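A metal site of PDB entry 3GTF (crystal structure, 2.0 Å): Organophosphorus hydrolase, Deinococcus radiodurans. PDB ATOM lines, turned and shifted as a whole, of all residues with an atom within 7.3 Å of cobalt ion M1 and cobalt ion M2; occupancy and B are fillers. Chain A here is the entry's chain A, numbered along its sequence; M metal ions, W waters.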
ATOM      1  N   HIS A  35      19.673  14.818   1.318  1.00  0.00           N
ATOM      2  CA  HIS A  35      18.455  14.219   0.781  1.00  0.00           C
ATOM      3  C   HIS A  35      17.199  14.784   1.461  1.00  0.00           C
ATOM      4  O   HIS A  35      16.791  14.314   2.509  1.00  0.00           O
ATOM      5  CB  HIS A  35      18.471  12.714   0.952  1.00  0.00           C
ATOM      6  CG  HIS A  35      17.318  12.012   0.289  1.00  0.00           C
ATOM      7  ND1 HIS A  35      17.490  10.867  -0.472  1.00  0.00           N
ATOM      8  CD2 HIS A  35      15.991  12.250   0.315  1.00  0.00           C
ATOM      9  CE1 HIS A  35      16.303  10.445  -0.887  1.00  0.00           C
ATOM     10  NE2 HIS A  35      15.381  11.271  -0.420  1.00  0.00           N
ATOM     11  N   GLU A  36      16.619  15.804   0.820  1.00  0.00           N
ATOM     12  CA  GLU A  36      15.403  16.478   1.282  1.00  0.00           C
ATOM     13  C   GLU A  36      14.512  16.771   0.054  1.00  0.00           C
ATOM     14  O   GLU A  36      14.939  16.662  -1.113  1.00  0.00           O
ATOM     15  CB  GLU A  36      15.765  17.817   1.952  1.00  0.00           C
ATOM     16  CG  GLU A  36      16.800  17.698   3.084  1.00  0.00           C
ATOM     17  CD  GLU A  36      16.278  16.968   4.293  1.00  0.00           C
ATOM     18  OE1 GLU A  36      17.102  16.439   5.056  1.00  0.00           O
ATOM     19  OE2 GLU A  36      15.055  16.933   4.494  1.00  0.00           O
ATOM     20  N   HIS A  37      13.274  17.164   0.312  1.00  0.00           N
ATOM     21  CA  HIS A  37      12.382  17.525  -0.773  1.00  0.00           C
ATOM     22  C   HIS A  37      11.669  18.845  -0.411  1.00  0.00           C
ATOM     23  O   HIS A  37      10.849  18.865   0.530  1.00  0.00           O
ATOM     24  CB  HIS A  37      11.343  16.439  -0.934  1.00  0.00           C
ATOM     25  CG  HIS A  37      11.915  15.110  -1.281  1.00  0.00           C
ATOM     26  ND1 HIS A  37      12.395  14.804  -2.536  1.00  0.00           N
ATOM     27  CD2 HIS A  37      12.093  13.998  -0.523  1.00  0.00           C
ATOM     28  CE1 HIS A  37      12.830  13.560  -2.547  1.00  0.00           C
ATOM     29  NE2 HIS A  37      12.671  13.055  -1.335  1.00  0.00           N
ATOM     30  N   PHE A  40       7.030  18.108  -2.960  1.00  0.00           N
ATOM     31  CA  PHE A  40       6.980  16.732  -3.400  1.00  0.00           C
ATOM     32  C   PHE A  40       5.547  16.267  -3.447  1.00  0.00           C
ATOM     33  O   PHE A  40       4.725  16.669  -2.627  1.00  0.00           O
ATOM     34  CB  PHE A  40       7.776  15.865  -2.425  1.00  0.00           C
ATOM     35  CG  PHE A  40       7.770  14.401  -2.768  1.00  0.00           C
ATOM     36  CD1 PHE A  40       6.712  13.570  -2.383  1.00  0.00           C
ATOM     37  CD2 PHE A  40       8.857  13.827  -3.432  1.00  0.00           C
ATOM     38  CE1 PHE A  40       6.726  12.207  -2.657  1.00  0.00           C
ATOM     39  CE2 PHE A  40       8.871  12.428  -3.726  1.00  0.00           C
ATOM     40  CZ  PHE A  40       7.806  11.632  -3.328  1.00  0.00           C
ATOM     41  N   ALA A  81      16.254  15.568  -3.679  1.00  0.00           N
ATOM     42  CA  ALA A  81      16.231  14.285  -4.361  1.00  0.00           C
ATOM     43  C   ALA A  81      14.902  13.912  -5.053  1.00  0.00           C
ATOM     44  O   ALA A  81      14.685  12.728  -5.419  1.00  0.00           O
ATOM     45  CB  ALA A  81      16.607  13.211  -3.394  1.00  0.00           C
ATOM     46  N   THR A  82      14.047  14.897  -5.255  1.00  0.00           N
ATOM     47  CA  THR A  82      12.743  14.659  -5.908  1.00  0.00           C
ATOM     48  C   THR A  82      12.852  14.161  -7.356  1.00  0.00           C
ATOM     49  O   THR A  82      13.468  14.809  -8.172  1.00  0.00           O
ATOM     50  CB  THR A  82      11.910  15.986  -5.906  1.00  0.00           C
ATOM     51  OG1 THR A  82      11.878  16.501  -4.557  1.00  0.00           O
ATOM     52  CG2 THR A  82      10.451  15.749  -6.385  1.00  0.00           C
ATOM     53  N   PRO A  83      12.282  12.983  -7.667  1.00  0.00           N
ATOM     54  CA  PRO A  83      12.279  12.394  -9.019  1.00  0.00           C
ATOM     55  C   PRO A  83      11.504  13.290  -9.964  1.00  0.00           C
ATOM     56  O   PRO A  83      10.585  13.973  -9.532  1.00  0.00           O
ATOM     57  CB  PRO A  83      11.564  11.074  -8.833  1.00  0.00           C
ATOM     58  CG  PRO A  83      11.926  10.698  -7.404  1.00  0.00           C
ATOM     59  CD  PRO A  83      11.921  11.970  -6.646  1.00  0.00           C
ATOM     60  N   TYR A 111      11.357   7.319  -9.905  1.00  0.00           N
ATOM     61  CA  TYR A 111      11.246   6.559  -8.685  1.00  0.00           C
ATOM     62  C   TYR A 111      11.270   5.038  -8.853  1.00  0.00           C
ATOM     63  O   TYR A 111      11.315   4.538  -9.986  1.00  0.00           O
ATOM     64  CB  TYR A 111       9.993   6.989  -7.926  1.00  0.00           C
ATOM     65  CG  TYR A 111      10.239   7.058  -6.445  1.00  0.00           C
ATOM     66  CD1 TYR A 111      11.553   7.144  -5.979  1.00  0.00           C
ATOM     67  CD2 TYR A 111       9.199   7.112  -5.522  1.00  0.00           C
ATOM     68  CE1 TYR A 111      11.833   7.294  -4.628  1.00  0.00           C
ATOM     69  CE2 TYR A 111       9.479   7.275  -4.160  1.00  0.00           C
ATOM     70  CZ  TYR A 111      10.799   7.362  -3.731  1.00  0.00           C
ATOM     71  OH  TYR A 111      11.114   7.549  -2.397  1.00  0.00           O
ATOM     72  N   TYR A 112      11.243   4.303  -7.741  1.00  0.00           N
ATOM     73  CA  TYR A 112      11.273   2.842  -7.800  1.00  0.00           C
ATOM     74  C   TYR A 112       9.982   2.325  -8.417  1.00  0.00           C
ATOM     75  O   TYR A 112       8.950   2.986  -8.375  1.00  0.00           O
ATOM     76  CB  TYR A 112      11.554   2.237  -6.414  1.00  0.00           C
ATOM     77  CG  TYR A 112      10.423   2.249  -5.400  1.00  0.00           C
ATOM     78  CD1 TYR A 112       9.725   1.073  -5.098  1.00  0.00           C
ATOM     79  CD2 TYR A 112      10.066   3.427  -4.736  1.00  0.00           C
ATOM     80  CE1 TYR A 112       8.714   1.063  -4.144  1.00  0.00           C
ATOM     81  CE2 TYR A 112       9.048   3.434  -3.794  1.00  0.00           C
ATOM     82  CZ  TYR A 112       8.386   2.257  -3.499  1.00  0.00           C
ATOM     83  OH  TYR A 112       7.418   2.245  -2.514  1.00  0.00           O
ATOM     84  N   KCX A 157      19.303  10.625  -9.343  1.00  0.00           N
ATOM     85  CA  KCX A 157      18.597   9.897  -8.310  1.00  0.00           C
ATOM     86  CB  KCX A 157      17.384  10.749  -7.799  1.00  0.00           C
ATOM     87  CG  KCX A 157      16.296  10.032  -6.932  1.00  0.00           C
ATOM     88  CD  KCX A 157      16.851   9.560  -5.572  1.00  0.00           C
ATOM     89  CE  KCX A 157      15.760   8.925  -4.667  1.00  0.00           C
ATOM     90  NZ  KCX A 157      14.799   9.940  -4.227  1.00  0.00           N
ATOM     91  C   KCX A 157      18.164   8.556  -8.906  1.00  0.00           C
ATOM     92  O   KCX A 157      17.550   8.501  -9.983  1.00  0.00           O
ATOM     93  CX  KCX A 157      13.912   9.743  -3.245  1.00  0.00           C
ATOM     94  OQ1 KCX A 157      13.927   8.696  -2.542  1.00  0.00           O
ATOM     95  OQ2 KCX A 157      13.116  10.662  -2.903  1.00  0.00           O
ATOM     96  N   LEU A 158      18.476   7.486  -8.195  1.00  0.00           N
ATOM     97  CA  LEU A 158      18.158   6.115  -8.594  1.00  0.00           C
ATOM     98  C   LEU A 158      17.329   5.502  -7.467  1.00  0.00           C
ATOM     99  O   LEU A 158      17.469   5.935  -6.329  1.00  0.00           O
ATOM    100  CB  LEU A 158      19.440   5.321  -8.768  1.00  0.00           C
ATOM    101  CG  LEU A 158      20.330   5.700  -9.965  1.00  0.00           C
ATOM    102  CD1 LEU A 158      21.532   4.701 -10.087  1.00  0.00           C
ATOM    103  CD2 LEU A 158      19.461   5.639 -11.247  1.00  0.00           C
ATOM    104  N   ALA A 159      16.450   4.541  -7.755  1.00  0.00           N
ATOM    105  CA  ALA A 159      15.629   3.922  -6.692  1.00  0.00           C
ATOM    106  C   ALA A 159      15.326   2.456  -7.022  1.00  0.00           C
ATOM    107  O   ALA A 159      15.099   2.125  -8.157  1.00  0.00           O
ATOM    108  CB  ALA A 159      14.312   4.697  -6.550  1.00  0.00           C
ATOM    109  N   THR A 189      20.814   7.344  -3.953  1.00  0.00           N
ATOM    110  CA  THR A 189      19.780   6.398  -4.173  1.00  0.00           C
ATOM    111  C   THR A 189      18.764   6.279  -3.037  1.00  0.00           C
ATOM    112  O   THR A 189      18.952   6.818  -1.934  1.00  0.00           O
ATOM    113  CB  THR A 189      20.381   5.012  -4.461  1.00  0.00           C
ATOM    114  OG1 THR A 189      20.790   4.377  -3.241  1.00  0.00           O
ATOM    115  CG2 THR A 189      21.580   5.167  -5.313  1.00  0.00           C
ATOM    116  N   HIS A 190      17.682   5.573  -3.363  1.00  0.00           N
ATOM    117  CA  HIS A 190      16.621   5.262  -2.448  1.00  0.00           C
ATOM    118  C   HIS A 190      16.680   3.745  -2.404  1.00  0.00           C
ATOM    119  O   HIS A 190      16.877   3.105  -3.450  1.00  0.00           O
ATOM    120  CB  HIS A 190      15.268   5.727  -3.057  1.00  0.00           C
ATOM    121  CG  HIS A 190      14.060   4.955  -2.592  1.00  0.00           C
ATOM    122  ND1 HIS A 190      13.044   5.528  -1.855  1.00  0.00           N
ATOM    123  CD2 HIS A 190      13.633   3.683  -2.878  1.00  0.00           C
ATOM    124  CE1 HIS A 190      12.050   4.669  -1.703  1.00  0.00           C
ATOM    125  NE2 HIS A 190      12.384   3.536  -2.313  1.00  0.00           N
ATOM    126  N   THR A 191      16.579   3.176  -1.205  1.00  0.00           N
ATOM    127  CA  THR A 191      16.474   1.731  -1.071  1.00  0.00           C
ATOM    128  C   THR A 191      15.105   1.598  -0.401  1.00  0.00           C
ATOM    129  O   THR A 191      14.706   2.458   0.397  1.00  0.00           O
ATOM    130  CB  THR A 191      17.555   1.100  -0.164  1.00  0.00           C
ATOM    131  OG1 THR A 191      17.577   1.770   1.101  1.00  0.00           O
ATOM    132  CG2 THR A 191      18.912   1.167  -0.847  1.00  0.00           C
ATOM    133  N   GLN A 192      14.384   0.542  -0.751  1.00  0.00           N
ATOM    134  CA  GLN A 192      13.059   0.316  -0.202  1.00  0.00           C
ATOM    135  C   GLN A 192      13.128  -0.625   0.985  1.00  0.00           C
ATOM    136  O   GLN A 192      13.814  -1.647   0.932  1.00  0.00           O
ATOM    137  CB  GLN A 192      12.187  -0.302  -1.281  1.00  0.00           C
ATOM    138  CG  GLN A 192      10.786  -0.612  -0.849  1.00  0.00           C
ATOM    139  CD  GLN A 192       9.969   0.646  -0.596  1.00  0.00           C
ATOM    140  OE1 GLN A 192      10.327   1.771  -0.988  1.00  0.00           O
ATOM    141  NE2 GLN A 192       8.834   0.451   0.056  1.00  0.00           N
ATOM    142  N   GLY A 217      21.138   5.429  -0.371  1.00  0.00           N
ATOM    143  CA  GLY A 217      20.220   6.032   0.592  1.00  0.00           C
ATOM    144  C   GLY A 217      19.284   5.140   1.367  1.00  0.00           C
ATOM    145  O   GLY A 217      19.174   3.923   1.106  1.00  0.00           O
ATOM    146  N   HIS A 218      18.578   5.770   2.296  1.00  0.00           N
ATOM    147  CA  HIS A 218      17.630   5.092   3.183  1.00  0.00           C
ATOM    148  C   HIS A 218      18.270   3.912   3.880  1.00  0.00           C
ATOM    149  O   HIS A 218      17.597   2.948   4.200  1.00  0.00           O
ATOM    150  CB  HIS A 218      16.402   4.613   2.432  1.00  0.00           C
ATOM    151  CG  HIS A 218      15.765   5.681   1.618  1.00  0.00           C
ATOM    152  ND1 HIS A 218      15.999   7.013   1.836  1.00  0.00           N
ATOM    153  CD2 HIS A 218      14.854   5.608   0.617  1.00  0.00           C
ATOM    154  CE1 HIS A 218      15.263   7.732   1.003  1.00  0.00           C
ATOM    155  NE2 HIS A 218      14.565   6.904   0.257  1.00  0.00           N
ATOM    156  N   ASP A 241      19.137   8.607   5.894  1.00  0.00           N
ATOM    157  CA  ASP A 241      18.489   9.820   5.445  1.00  0.00           C
ATOM    158  C   ASP A 241      17.041  10.088   5.675  1.00  0.00           C
ATOM    159  O   ASP A 241      16.471  10.964   5.035  1.00  0.00           O
ATOM    160  CB  ASP A 241      18.823  10.076   3.977  1.00  0.00           C
ATOM    161  CG  ASP A 241      18.429   8.936   3.080  1.00  0.00           C
ATOM    162  OD1 ASP A 241      18.874   8.930   1.908  1.00  0.00           O
ATOM    163  OD2 ASP A 241      17.683   8.042   3.557  1.00  0.00           O
ATOM    164  N   ARG A 242      16.427   9.348   6.572  1.00  0.00           N
ATOM    165  CA  ARG A 242      15.042   9.645   6.832  1.00  0.00           C
ATOM    166  C   ARG A 242      14.954   9.801   8.354  1.00  0.00           C
ATOM    167  O   ARG A 242      14.010   9.304   8.982  1.00  0.00           O
ATOM    168  CB  ARG A 242      14.181   8.488   6.346  1.00  0.00           C
ATOM    169  CG  ARG A 242      14.471   8.111   4.911  1.00  0.00           C
ATOM    170  CD  ARG A 242      13.525   7.012   4.454  1.00  0.00           C
ATOM    171  NE  ARG A 242      12.275   7.584   3.970  1.00  0.00           N
ATOM    172  CZ  ARG A 242      11.165   6.873   3.748  1.00  0.00           C
ATOM    173  NH1 ARG A 242      11.163   5.576   3.967  1.00  0.00           N
ATOM    174  NH2 ARG A 242      10.064   7.470   3.309  1.00  0.00           N
ATOM    175  N   HIS A 277      16.970  13.942   6.434  1.00  0.00           N
ATOM    176  CA  HIS A 277      15.632  13.653   6.941  1.00  0.00           C
ATOM    177  C   HIS A 277      14.652  13.145   5.855  1.00  0.00           C
ATOM    178  O   HIS A 277      13.653  12.536   6.176  1.00  0.00           O
ATOM    179  CB  HIS A 277      14.963  14.906   7.598  1.00  0.00           C
ATOM    180  CG  HIS A 277      15.900  15.798   8.372  1.00  0.00           C
ATOM    181  ND1 HIS A 277      15.971  15.795   9.747  1.00  0.00           N
ATOM    182  CD2 HIS A 277      16.735  16.771   7.956  1.00  0.00           C
ATOM    183  CE1 HIS A 277      16.829  16.714  10.155  1.00  0.00           C
ATOM    184  NE2 HIS A 277      17.304  17.325   9.086  1.00  0.00           N
ATOM    185  N   ASP A 278      14.914  13.430   4.584  1.00  0.00           N
ATOM    186  CA  ASP A 278      13.981  13.050   3.516  1.00  0.00           C
ATOM    187  C   ASP A 278      12.651  13.773   3.819  1.00  0.00           C
ATOM    188  O   ASP A 278      11.566  13.238   3.594  1.00  0.00           O
ATOM    189  CB  ASP A 278      13.772  11.531   3.530  1.00  0.00           C
ATOM    190  CG  ASP A 278      13.011  11.035   2.318  1.00  0.00           C
ATOM    191  OD1 ASP A 278      12.511   9.886   2.351  1.00  0.00           O
ATOM    192  OD2 ASP A 278      12.924  11.793   1.346  1.00  0.00           O
ATOM    193  N   SER A 279      12.725  15.004   4.333  1.00  0.00           N
ATOM    194  CA  SER A 279      11.508  15.743   4.690  1.00  0.00           C
ATOM    195  C   SER A 279      10.864  16.412   3.497  1.00  0.00           C
ATOM    196  O   SER A 279      11.509  16.663   2.500  1.00  0.00           O
ATOM    197  CB  SER A 279      11.825  16.819   5.742  1.00  0.00           C
ATOM    198  OG  SER A 279      12.510  17.910   5.155  1.00  0.00           O
ATOM    199  N   ILE A 280       9.557  16.690   3.594  1.00  0.00           N
ATOM    200  CA  ILE A 280       8.857  17.390   2.525  1.00  0.00           C
ATOM    201  C   ILE A 280       8.469  18.728   3.132  1.00  0.00           C
ATOM    202  O   ILE A 280       7.683  18.787   4.099  1.00  0.00           O
ATOM    203  CB  ILE A 280       7.570  16.645   2.069  1.00  0.00           C
ATOM    204  CG1 ILE A 280       7.943  15.353   1.361  1.00  0.00           C
ATOM    205  CG2 ILE A 280       6.774  17.513   1.094  1.00  0.00           C
ATOM    206  CD1 ILE A 280       7.833  14.162   2.233  1.00  0.00           C
HETATM  207 CO    CO M   1      13.024   7.577  -1.167  1.00  0.00          CO
HETATM  208 CO    CO M   2      13.113  11.176  -0.808  1.00  0.00          CO
HETATM  209  O   HOH W   1      12.580   9.597  -0.080  1.00  0.00           O
HETATM  210  O   HOH W   2      11.424   6.948   0.435  1.00  0.00           O
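N of His 37 sits at hydrogen-bond distance from O of Ser 279 (2.9 Å). The side-chain carboxylate (OD2) of Asp 241 lies within hydrogen-bond range of a ring nitrogen (ND1) of His 218, at 2.6 Å. A ring nitrogen (ND1) of His 37 lies within hydrogen-bond range of the side-chain hydroxyl of Thr 82, 2.7 Å away. O of His 218 is in hydrogen-bond range of OG1 of Thr 191 (3.3 Å). OD1 of Asp 278 lies within salt-bridge range of NE of Arg 242 (2.8 Å). The backbone carbonyl oxygen (O) of Leu 158 sits at hydrogen-bond distance from the backbone NH (N) of His 190 (3.0 Å). A ring nitrogen (NE2) of His 190 lies within hydrogen-bond range of the side-chain amide oxygen of Gln 192, 3.0 Å away. ND1 of His 35 is in hydrogen-bond range of OD1 of Asp 241 (3.4 Å).
Within 4 Å of cobalt ion M2: His 35, His 37, KCX 157 and Asp 278.
Cobalt ion M1 is bound by OQ1 of KCX 157 (2.0 Å), ND1 of His 190 (2.2 Å), NE2 of His 218 (2.2 Å), OH of Tyr 111 (2.3 Å), water W1 (2.3 Å) and water W2 (2.3 Å).
Cobalt ion M2 is bound by water W1 (1.8 Å), NE2 of His 37 (2.0 Å), OQ2 of KCX 157 (2.2 Å), OD2 of Asp 278 (2.2 Å) and NE2 of His 35 (2.3 Å).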
